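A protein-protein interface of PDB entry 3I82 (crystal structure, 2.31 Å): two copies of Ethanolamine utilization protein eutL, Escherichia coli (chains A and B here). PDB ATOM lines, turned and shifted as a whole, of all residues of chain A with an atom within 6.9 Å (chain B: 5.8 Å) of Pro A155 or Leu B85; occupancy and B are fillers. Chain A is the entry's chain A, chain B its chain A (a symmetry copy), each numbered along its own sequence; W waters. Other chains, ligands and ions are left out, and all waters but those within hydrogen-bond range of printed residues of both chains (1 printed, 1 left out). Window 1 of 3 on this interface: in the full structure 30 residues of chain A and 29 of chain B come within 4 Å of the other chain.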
ATOM      1  N   ALA A 153      -5.814  -8.530  32.154  1.00  0.00           N
ATOM      2  CA  ALA A 153      -4.586  -9.134  31.634  1.00  0.00           C
ATOM      3  C   ALA A 153      -4.937 -10.258  30.683  1.00  0.00           C
ATOM      4  O   ALA A 153      -6.096 -10.679  30.627  1.00  0.00           O
ATOM      5  CB  ALA A 153      -3.713  -9.652  32.777  1.00  0.00           C
ATOM      6  N   PRO A 154      -3.954 -10.768  29.926  1.00  0.00           N
ATOM      7  CA  PRO A 154      -4.262 -11.867  29.019  1.00  0.00           C
ATOM      8  C   PRO A 154      -4.776 -13.071  29.808  1.00  0.00           C
ATOM      9  O   PRO A 154      -4.434 -13.241  30.974  1.00  0.00           O
ATOM     10  CB  PRO A 154      -2.926 -12.143  28.321  1.00  0.00           C
ATOM     11  CG  PRO A 154      -2.258 -10.808  28.331  1.00  0.00           C
ATOM     12  CD  PRO A 154      -2.565 -10.301  29.721  1.00  0.00           C
ATOM     13  N   PRO A 155      -5.562 -13.936  29.168  1.00  0.00           N
ATOM     14  CA  PRO A 155      -6.191 -15.095  29.811  1.00  0.00           C
ATOM     15  C   PRO A 155      -5.483 -15.738  31.006  1.00  0.00           C
ATOM     16  O   PRO A 155      -6.026 -15.743  32.109  1.00  0.00           O
ATOM     17  CB  PRO A 155      -6.370 -16.076  28.655  1.00  0.00           C
ATOM     18  CG  PRO A 155      -6.608 -15.171  27.491  1.00  0.00           C
ATOM     19  CD  PRO A 155      -5.605 -14.067  27.697  1.00  0.00           C
ATOM     20  N   LEU A 156      -4.277 -16.256  30.803  1.00  0.00           N
ATOM     21  CA  LEU A 156      -3.579 -16.961  31.882  1.00  0.00           C
ATOM     22  C   LEU A 156      -3.054 -16.034  32.980  1.00  0.00           C
ATOM     23  O   LEU A 156      -3.195 -16.329  34.168  1.00  0.00           O
ATOM     24  CB  LEU A 156      -2.443 -17.834  31.321  1.00  0.00           C
ATOM     25  CG  LEU A 156      -1.962 -18.956  32.260  1.00  0.00           C
ATOM     26  CD1 LEU A 156      -1.427 -20.139  31.472  1.00  0.00           C
ATOM     27  CD2 LEU A 156      -0.916 -18.428  33.230  1.00  0.00           C
ATOM     28  N   GLU A 157      -2.433 -14.935  32.570  1.00  0.00           N
ATOM     29  CA  GLU A 157      -1.899 -13.935  33.493  1.00  0.00           C
ATOM     30  C   GLU A 157      -3.028 -13.453  34.395  1.00  0.00           C
ATOM     31  O   GLU A 157      -2.860 -13.343  35.608  1.00  0.00           O
ATOM     32  CB  GLU A 157      -1.313 -12.731  32.727  1.00  0.00           C
ATOM     33  CG  GLU A 157       0.118 -12.910  32.177  1.00  0.00           C
ATOM     34  CD  GLU A 157       0.176 -13.565  30.800  1.00  0.00           C
ATOM     35  OE1 GLU A 157      -0.729 -14.384  30.505  1.00  0.00           O
ATOM     36  OE2 GLU A 157       1.138 -13.272  30.053  1.00  0.00           O
ATOM     37  N   ALA A 158      -4.181 -13.187  33.790  1.00  0.00           N
ATOM     38  CA  ALA A 158      -5.355 -12.711  34.510  1.00  0.00           C
ATOM     39  C   ALA A 158      -5.885 -13.721  35.517  1.00  0.00           C
ATOM     40  O   ALA A 158      -6.173 -13.362  36.654  1.00  0.00           O
ATOM     41  CB  ALA A 158      -6.455 -12.336  33.523  1.00  0.00           C
ATOM     42  N   THR A 159      -6.020 -14.978  35.107  1.00  0.00           N
ATOM     43  CA  THR A 159      -6.525 -16.023  36.014  1.00  0.00           C
ATOM     44  C   THR A 159      -5.602 -16.199  37.221  1.00  0.00           C
ATOM     45  O   THR A 159      -6.055 -16.200  38.378  1.00  0.00           O
ATOM     46  CB  THR A 159      -6.663 -17.393  35.298  1.00  0.00           C
ATOM     47  OG1 THR A 159      -7.322 -17.211  34.042  1.00  0.00           O
ATOM     48  CG2 THR A 159      -7.504 -18.365  36.128  1.00  0.00           C
ATOM     49  N   TYR A 160      -4.310 -16.340  36.941  1.00  0.00           N
ATOM     50  CA  TYR A 160      -3.299 -16.499  37.985  1.00  0.00           C
ATOM     51  C   TYR A 160      -3.292 -15.284  38.910  1.00  0.00           C
ATOM     52  O   TYR A 160      -3.315 -15.420  40.132  1.00  0.00           O
ATOM     53  CB  TYR A 160      -1.915 -16.679  37.355  1.00  0.00           C
ATOM     54  CG  TYR A 160      -0.859 -17.217  38.300  1.00  0.00           C
ATOM     55  CD1 TYR A 160      -0.895 -18.541  38.731  1.00  0.00           C
ATOM     56  CD2 TYR A 160       0.180 -16.404  38.763  1.00  0.00           C
ATOM     57  CE1 TYR A 160       0.078 -19.046  39.586  1.00  0.00           C
ATOM     58  CE2 TYR A 160       1.159 -16.901  39.616  1.00  0.00           C
ATOM     59  CZ  TYR A 160       1.097 -18.220  40.026  1.00  0.00           C
ATOM     60  OH  TYR A 160       2.066 -18.717  40.868  1.00  0.00           O
ATOM     61  N   TYR A 176     -16.446 -11.060  37.440  1.00  0.00           N
ATOM     62  CA  TYR A 176     -15.392 -11.789  36.774  1.00  0.00           C
ATOM     63  C   TYR A 176     -15.786 -12.018  35.322  1.00  0.00           C
ATOM     64  O   TYR A 176     -16.815 -12.639  35.024  1.00  0.00           O
ATOM     65  CB  TYR A 176     -15.123 -13.125  37.475  1.00  0.00           C
ATOM     66  CG  TYR A 176     -14.152 -14.019  36.721  1.00  0.00           C
ATOM     67  CD1 TYR A 176     -14.460 -15.360  36.475  1.00  0.00           C
ATOM     68  CD2 TYR A 176     -12.930 -13.530  36.261  1.00  0.00           C
ATOM     69  CE1 TYR A 176     -13.582 -16.190  35.791  1.00  0.00           C
ATOM     70  CE2 TYR A 176     -12.041 -14.352  35.578  1.00  0.00           C
ATOM     71  CZ  TYR A 176     -12.369 -15.676  35.351  1.00  0.00           C
ATOM     72  OH  TYR A 176     -11.477 -16.473  34.672  1.00  0.00           O
ATOM     73  N   PRO A 179     -11.938 -15.229  30.009  1.00  0.00           N
ATOM     74  CA  PRO A 179     -11.429 -15.038  28.651  1.00  0.00           C
ATOM     75  C   PRO A 179     -12.217 -15.817  27.587  1.00  0.00           C
ATOM     76  O   PRO A 179     -12.625 -16.951  27.820  1.00  0.00           O
ATOM     77  CB  PRO A 179      -9.992 -15.536  28.760  1.00  0.00           C
ATOM     78  CG  PRO A 179     -10.096 -16.634  29.765  1.00  0.00           C
ATOM     79  CD  PRO A 179     -11.050 -16.098  30.802  1.00  0.00           C
ATOM     80  N   PRO A 180     -12.412 -15.220  26.399  1.00  0.00           N
ATOM     81  CA  PRO A 180     -11.936 -13.889  26.049  1.00  0.00           C
ATOM     82  C   PRO A 180     -13.020 -12.823  26.074  1.00  0.00           C
ATOM     83  O   PRO A 180     -14.216 -13.131  25.964  1.00  0.00           O
ATOM     84  CB  PRO A 180     -11.453 -14.081  24.622  1.00  0.00           C
ATOM     85  CG  PRO A 180     -12.514 -14.969  24.056  1.00  0.00           C
ATOM     86  CD  PRO A 180     -12.861 -15.938  25.192  1.00  0.00           C
ATOM     87  N   ASN A 184      -9.810 -10.060  23.722  1.00  0.00           N
ATOM     88  CA  ASN A 184      -9.003 -11.237  24.059  1.00  0.00           C
ATOM     89  C   ASN A 184      -8.217 -11.096  25.357  1.00  0.00           C
ATOM     90  O   ASN A 184      -7.154 -11.704  25.520  1.00  0.00           O
ATOM     91  CB  ASN A 184      -8.067 -11.624  22.903  1.00  0.00           C
ATOM     92  CG  ASN A 184      -8.824 -12.092  21.679  1.00  0.00           C
ATOM     93  OD1 ASN A 184      -9.766 -12.878  21.788  1.00  0.00           O
ATOM     94  ND2 ASN A 184      -8.404 -11.636  20.502  1.00  0.00           N
ATOM     95  N   TYR A 185      -8.741 -10.288  26.269  1.00  0.00           N
ATOM     96  CA  TYR A 185      -8.167 -10.163  27.595  1.00  0.00           C
ATOM     97  C   TYR A 185      -9.188 -10.754  28.555  1.00  0.00           C
ATOM     98  O   TYR A 185     -10.289 -11.148  28.150  1.00  0.00           O
ATOM     99  CB  TYR A 185      -7.917  -8.701  27.964  1.00  0.00           C
ATOM    100  CG  TYR A 185      -6.678  -8.097  27.340  1.00  0.00           C
ATOM    101  CD1 TYR A 185      -5.513  -7.938  28.079  1.00  0.00           C
ATOM    102  CD2 TYR A 185      -6.672  -7.693  26.007  1.00  0.00           C
ATOM    103  CE1 TYR A 185      -4.372  -7.385  27.508  1.00  0.00           C
ATOM    104  CE2 TYR A 185      -5.543  -7.142  25.429  1.00  0.00           C
ATOM    105  CZ  TYR A 185      -4.396  -6.993  26.177  1.00  0.00           C
ATOM    106  OH  TYR A 185      -3.283  -6.438  25.589  1.00  0.00           O
ATOM    107  N   SER A 186      -8.810 -10.819  29.824  1.00  0.00           N
ATOM    108  CA  SER A 186      -9.696 -11.286  30.877  1.00  0.00           C
ATOM    109  C   SER A 186      -9.702 -10.173  31.920  1.00  0.00           C
ATOM    110  O   SER A 186      -8.725  -9.429  32.040  1.00  0.00           O
ATOM    111  CB  SER A 186      -9.190 -12.593  31.473  1.00  0.00           C
ATOM    112  OG  SER A 186     -10.274 -13.270  32.097  1.00  0.00           O
ATOM    113  N   LEU B  39      -3.227 -24.121  34.852  1.00  0.00           N
ATOM    114  CA  LEU B  39      -3.527 -23.216  33.740  1.00  0.00           C
ATOM    115  C   LEU B  39      -2.514 -23.389  32.627  1.00  0.00           C
ATOM    116  O   LEU B  39      -1.312 -23.450  32.888  1.00  0.00           O
ATOM    117  CB  LEU B  39      -3.465 -21.765  34.202  1.00  0.00           C
ATOM    118  CG  LEU B  39      -4.115 -21.475  35.551  1.00  0.00           C
ATOM    119  CD1 LEU B  39      -3.745 -20.072  36.006  1.00  0.00           C
ATOM    120  CD2 LEU B  39      -5.627 -21.670  35.449  1.00  0.00           C
ATOM    121  N   ILE B  40      -2.988 -23.435  31.388  1.00  0.00           N
ATOM    122  CA  ILE B  40      -2.076 -23.541  30.266  1.00  0.00           C
ATOM    123  C   ILE B  40      -2.621 -22.856  29.023  1.00  0.00           C
ATOM    124  O   ILE B  40      -3.816 -22.931  28.701  1.00  0.00           O
ATOM    125  CB  ILE B  40      -1.745 -25.013  29.953  1.00  0.00           C
ATOM    126  CG1 ILE B  40      -0.645 -25.086  28.886  1.00  0.00           C
ATOM    127  CG2 ILE B  40      -3.011 -25.770  29.550  1.00  0.00           C
ATOM    128  CD1 ILE B  40      -0.014 -26.475  28.742  1.00  0.00           C
ATOM    129  N   SER B  41      -1.733 -22.168  28.318  1.00  0.00           N
ATOM    130  CA  SER B  41      -2.125 -21.507  27.080  1.00  0.00           C
ATOM    131  C   SER B  41      -1.219 -21.925  25.922  1.00  0.00           C
ATOM    132  O   SER B  41      -0.010 -22.088  26.086  1.00  0.00           O
ATOM    133  CB  SER B  41      -2.101 -19.988  27.257  1.00  0.00           C
ATOM    134  OG  SER B  41      -0.841 -19.526  27.714  1.00  0.00           O
ATOM    135  N   ALA B  42      -1.788 -22.086  24.731  1.00  0.00           N
ATOM    136  CA  ALA B  42      -1.000 -22.517  23.572  1.00  0.00           C
ATOM    137  C   ALA B  42      -1.403 -21.770  22.313  1.00  0.00           C
ATOM    138  O   ALA B  42      -2.443 -21.117  22.295  1.00  0.00           O
ATOM    139  CB  ALA B  42      -1.171 -24.012  23.365  1.00  0.00           C
ATOM    140  N   TYR B  49      -7.405 -28.595  22.734  1.00  0.00           N
ATOM    141  CA  TYR B  49      -8.633 -29.189  23.257  1.00  0.00           C
ATOM    142  C   TYR B  49      -8.457 -30.699  23.312  1.00  0.00           C
ATOM    143  O   TYR B  49      -8.877 -31.357  24.270  1.00  0.00           O
ATOM    144  CB  TYR B  49      -9.849 -28.806  22.397  1.00  0.00           C
ATOM    145  CG  TYR B  49     -10.233 -27.341  22.485  1.00  0.00           C
ATOM    146  CD1 TYR B  49     -10.253 -26.677  23.716  1.00  0.00           C
ATOM    147  CD2 TYR B  49     -10.581 -26.616  21.343  1.00  0.00           C
ATOM    148  CE1 TYR B  49     -10.607 -25.338  23.809  1.00  0.00           C
ATOM    149  CE2 TYR B  49     -10.940 -25.278  21.423  1.00  0.00           C
ATOM    150  CZ  TYR B  49     -10.947 -24.643  22.662  1.00  0.00           C
ATOM    151  OH  TYR B  49     -11.297 -23.316  22.766  1.00  0.00           O
ATOM    152  N   TYR B  65     -12.351 -25.119  32.542  1.00  0.00           N
ATOM    153  CA  TYR B  65     -12.616 -24.056  31.581  1.00  0.00           C
ATOM    154  C   TYR B  65     -11.838 -24.270  30.295  1.00  0.00           C
ATOM    155  O   TYR B  65     -10.685 -24.706  30.332  1.00  0.00           O
ATOM    156  CB  TYR B  65     -12.232 -22.687  32.172  1.00  0.00           C
ATOM    157  CG  TYR B  65     -12.735 -21.500  31.373  1.00  0.00           C
ATOM    158  CD1 TYR B  65     -14.033 -21.026  31.550  1.00  0.00           C
ATOM    159  CD2 TYR B  65     -11.922 -20.862  30.431  1.00  0.00           C
ATOM    160  CE1 TYR B  65     -14.515 -19.945  30.808  1.00  0.00           C
ATOM    161  CE2 TYR B  65     -12.396 -19.774  29.681  1.00  0.00           C
ATOM    162  CZ  TYR B  65     -13.693 -19.325  29.880  1.00  0.00           C
ATOM    163  OH  TYR B  65     -14.193 -18.262  29.158  1.00  0.00           O
ATOM    164  N   GLY B  66     -12.453 -23.915  29.170  1.00  0.00           N
ATOM    165  CA  GLY B  66     -11.812 -24.071  27.870  1.00  0.00           C
ATOM    166  C   GLY B  66     -12.462 -23.178  26.833  1.00  0.00           C
ATOM    167  O   GLY B  66     -13.608 -23.401  26.439  1.00  0.00           O
ATOM    168  N   ARG B  67     -11.726 -22.160  26.398  1.00  0.00           N
ATOM    169  CA  ARG B  67     -12.217 -21.213  25.401  1.00  0.00           C
ATOM    170  C   ARG B  67     -11.074 -20.652  24.544  1.00  0.00           C
ATOM    171  O   ARG B  67      -9.947 -20.450  25.021  1.00  0.00           O
ATOM    172  CB  ARG B  67     -12.964 -20.057  26.077  1.00  0.00           C
ATOM    173  CG  ARG B  67     -13.858 -19.274  25.122  1.00  0.00           C
ATOM    174  CD  ARG B  67     -15.322 -19.693  25.204  1.00  0.00           C
ATOM    175  NE  ARG B  67     -16.104 -18.707  25.946  1.00  0.00           N
ATOM    176  CZ  ARG B  67     -16.480 -17.525  25.462  1.00  0.00           C
ATOM    177  NH1 ARG B  67     -16.162 -17.176  24.218  1.00  0.00           N
ATOM    178  NH2 ARG B  67     -17.181 -16.692  26.227  1.00  0.00           N
ATOM    179  N   SER B  68     -11.400 -20.380  23.281  1.00  0.00           N
ATOM    180  CA  SER B  68     -10.451 -19.867  22.298  1.00  0.00           C
ATOM    181  C   SER B  68     -10.573 -18.355  22.102  1.00  0.00           C
ATOM    182  O   SER B  68     -11.575 -17.754  22.495  1.00  0.00           O
ATOM    183  CB  SER B  68     -10.652 -20.591  20.963  1.00  0.00           C
ATOM    184  OG  SER B  68     -11.937 -20.340  20.442  1.00  0.00           O
ATOM    185  N   LEU B  69      -9.553 -17.758  21.481  1.00  0.00           N
ATOM    186  CA  LEU B  69      -9.509 -16.307  21.268  1.00  0.00           C
ATOM    187  C   LEU B  69      -9.972 -15.847  19.878  1.00  0.00           C
ATOM    188  O   LEU B  69      -9.791 -16.549  18.872  1.00  0.00           O
ATOM    189  CB  LEU B  69      -8.099 -15.775  21.544  1.00  0.00           C
ATOM    190  CG  LEU B  69      -7.437 -16.221  22.853  1.00  0.00           C
ATOM    191  CD1 LEU B  69      -6.095 -15.508  23.011  1.00  0.00           C
ATOM    192  CD2 LEU B  69      -8.333 -15.946  24.050  1.00  0.00           C
ATOM    193  N   PRO B  77      -3.317 -10.862  21.616  1.00  0.00           N
ATOM    194  CA  PRO B  77      -2.898  -9.662  22.338  1.00  0.00           C
ATOM    195  C   PRO B  77      -1.462  -9.743  22.864  1.00  0.00           C
ATOM    196  O   PRO B  77      -0.854  -8.708  23.135  1.00  0.00           O
ATOM    197  CB  PRO B  77      -3.900  -9.596  23.483  1.00  0.00           C
ATOM    198  CG  PRO B  77      -4.100 -11.031  23.807  1.00  0.00           C
ATOM    199  CD  PRO B  77      -4.223 -11.679  22.441  1.00  0.00           C
ATOM    200  N   ALA B  81      -0.562 -15.451  25.210  1.00  0.00           N
ATOM    201  CA  ALA B  81      -1.977 -15.760  24.992  1.00  0.00           C
ATOM    202  C   ALA B  81      -2.236 -16.922  24.031  1.00  0.00           C
ATOM    203  O   ALA B  81      -3.157 -17.719  24.250  1.00  0.00           O
ATOM    204  CB  ALA B  81      -2.718 -14.515  24.498  1.00  0.00           C
ATOM    205  N   GLU B  83      -3.941 -18.792  21.418  1.00  0.00           N
ATOM    206  CA  GLU B  83      -5.354 -18.638  21.054  1.00  0.00           C
ATOM    207  C   GLU B  83      -6.273 -19.535  21.901  1.00  0.00           C
ATOM    208  O   GLU B  83      -7.414 -19.815  21.519  1.00  0.00           O
ATOM    209  CB  GLU B  83      -5.555 -18.899  19.551  1.00  0.00           C
ATOM    210  CG  GLU B  83      -5.057 -20.242  19.066  1.00  0.00           C
ATOM    211  CD  GLU B  83      -5.444 -20.537  17.622  1.00  0.00           C
ATOM    212  OE1 GLU B  83      -5.925 -21.661  17.357  1.00  0.00           O
ATOM    213  OE2 GLU B  83      -5.274 -19.671  16.733  1.00  0.00           O
ATOM    214  N   VAL B  84      -5.761 -19.985  23.048  1.00  0.00           N
ATOM    215  CA  VAL B  84      -6.514 -20.828  23.979  1.00  0.00           C
ATOM    216  C   VAL B  84      -6.027 -20.743  25.408  1.00  0.00           C
ATOM    217  O   VAL B  84      -4.856 -20.472  25.671  1.00  0.00           O
ATOM    218  CB  VAL B  84      -6.437 -22.356  23.648  1.00  0.00           C
ATOM    219  CG1 VAL B  84      -7.728 -22.841  23.022  1.00  0.00           C
ATOM    220  CG2 VAL B  84      -5.205 -22.671  22.794  1.00  0.00           C
ATOM    221  N   LEU B  85      -6.952 -21.004  26.321  1.00  0.00           N
ATOM    222  CA  LEU B  85      -6.629 -21.157  27.729  1.00  0.00           C
ATOM    223  C   LEU B  85      -7.410 -22.361  28.232  1.00  0.00           C
ATOM    224  O   LEU B  85      -8.634 -22.434  28.072  1.00  0.00           O
ATOM    225  CB  LEU B  85      -7.006 -19.937  28.567  1.00  0.00           C
ATOM    226  CG  LEU B  85      -6.829 -20.181  30.078  1.00  0.00           C
ATOM    227  CD1 LEU B  85      -5.361 -20.442  30.402  1.00  0.00           C
ATOM    228  CD2 LEU B  85      -7.352 -18.999  30.883  1.00  0.00           C
ATOM    229  N   ILE B  86      -6.686 -23.312  28.807  1.00  0.00           N
ATOM    230  CA  ILE B  86      -7.307 -24.461  29.426  1.00  0.00           C
ATOM    231  C   ILE B  86      -7.026 -24.384  30.921  1.00  0.00           C
ATOM    232  O   ILE B  86      -5.906 -24.071  31.347  1.00  0.00           O
ATOM    233  CB  ILE B  86      -6.760 -25.800  28.873  1.00  0.00           C
ATOM    234  CG1 ILE B  86      -7.267 -26.031  27.440  1.00  0.00           C
ATOM    235  CG2 ILE B  86      -7.182 -26.959  29.789  1.00  0.00           C
ATOM    236  CD1 ILE B  86      -8.749 -26.358  27.339  1.00  0.00           C
ATOM    237  N   MET B  87      -8.066 -24.630  31.712  1.00  0.00           N
ATOM    238  CA  MET B  87      -7.935 -24.718  33.162  1.00  0.00           C
ATOM    239  C   MET B  87      -8.333 -26.143  33.519  1.00  0.00           C
ATOM    240  O   MET B  87      -9.498 -26.496  33.341  1.00  0.00           O
ATOM    241  CB  MET B  87      -8.877 -23.749  33.886  1.00  0.00           C
ATOM    242  CG  MET B  87      -8.626 -22.272  33.637  1.00  0.00           C
ATOM    243  SD  MET B  87      -9.717 -21.319  34.716  1.00  0.00           S
ATOM    244  CE  MET B  87     -10.019 -19.814  33.736  1.00  0.00           C
HETATM  245  O   HOH W   1      -1.066  -8.072  26.040  1.00  0.00           O
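The backbone carbonyl oxygen (O) of Pro A179 is in hydrogen-bond range of the side-chain hydroxyl (OH) of Tyr B65.
No position is printed for both chains.
Of the 19 pairs that touch across the chains among the printed residues, none has its exchanged pair printed and touching as well.
Among the printed residues, pairs that only touch across the chains: Pro A180 with Ser B68, Asn A184 with Leu B69, Pro A180 with Arg B67, Tyr A185 with Pro B77, Asn A184 with Pro B77, Pro A179 with Arg B67, Leu A156 with Leu B39, Thr A159 with Leu B85, Leu A156 with Ile B40, Pro A180 with Leu B69, Pro A155 with Leu B85, Thr A159 with Met B87, Leu A156 with Ser B41, Tyr A176 with Met B87, Pro A179 with Leu B85, Thr A159 with Leu B39, Tyr A160 with Leu B39 and Pro A155 with Leu B69.
Water W1 bridges OH of Tyr A185 (2.8 Å) and O of Pro B77 (3.0 Å).
Hydrophobic or aromatic side chains of chain A within 4 Å of the printed part of chain B: Pro A155, Leu A156, Tyr A176, Pro A179, Pro A180 and Tyr A185.
Of the 17 printed residues of chain B, 10 touch a printed residue of chain A.
Pro A155 touches just these residues of chain B: Leu B69 and Leu B85.
Glu A157 touches none of the printed residues of chain B.
Printed residues of chain B within 4 Å of Pro A179: Tyr B65, Arg B67 and Leu B85.
Of the printed residues of chain B, Tyr A185 touches Pro B77.
Printed residues of chain A within 4 Å of Leu B39: Leu A156 (3.6 Å), Thr A159 (3.9 Å) and Tyr A160 (3.9 Å).
Printed residues of chain A within 4 Å of Pro B77: Asn A184 (3.6 Å) and Tyr A185 (3.5 Å).
Ala B81 touches none of the printed residues of chain A.
Leu B85 touches just these residues of chain A: Pro A155 (3.7 Å), Thr A159 (3.6 Å) and Pro A179 (3.8 Å).
The nearest residue of chain B that does not touch Pro A155 is Ala B81 (4.3 Å).
The nearest residue of chain A that does not touch Leu B85 is Leu A156 (4.02 Å).
N of Met B87 sits at hydrogen-bond distance from O of Tyr B65, 3.0 Å away.
The backbone NH of Leu B69 lies within hydrogen-bond range of the backbone carbonyl oxygen of Glu B83 (3.0 Å).
N of Ile B86 is in hydrogen-bond range of O of Ile B40, 2.9 Å away.
The backbone NH of Ser B68 is in hydrogen-bond range of the side-chain hydroxyl of Tyr B49, 3.0 Å away.
O of Pro A155 is in hydrogen-bond range of OG1 of Thr A159, 2.8 Å away.
The backbone NH (N) of Leu B85 lies within hydrogen-bond range of the backbone carbonyl oxygen (O) of Arg B67 (3.3 Å).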
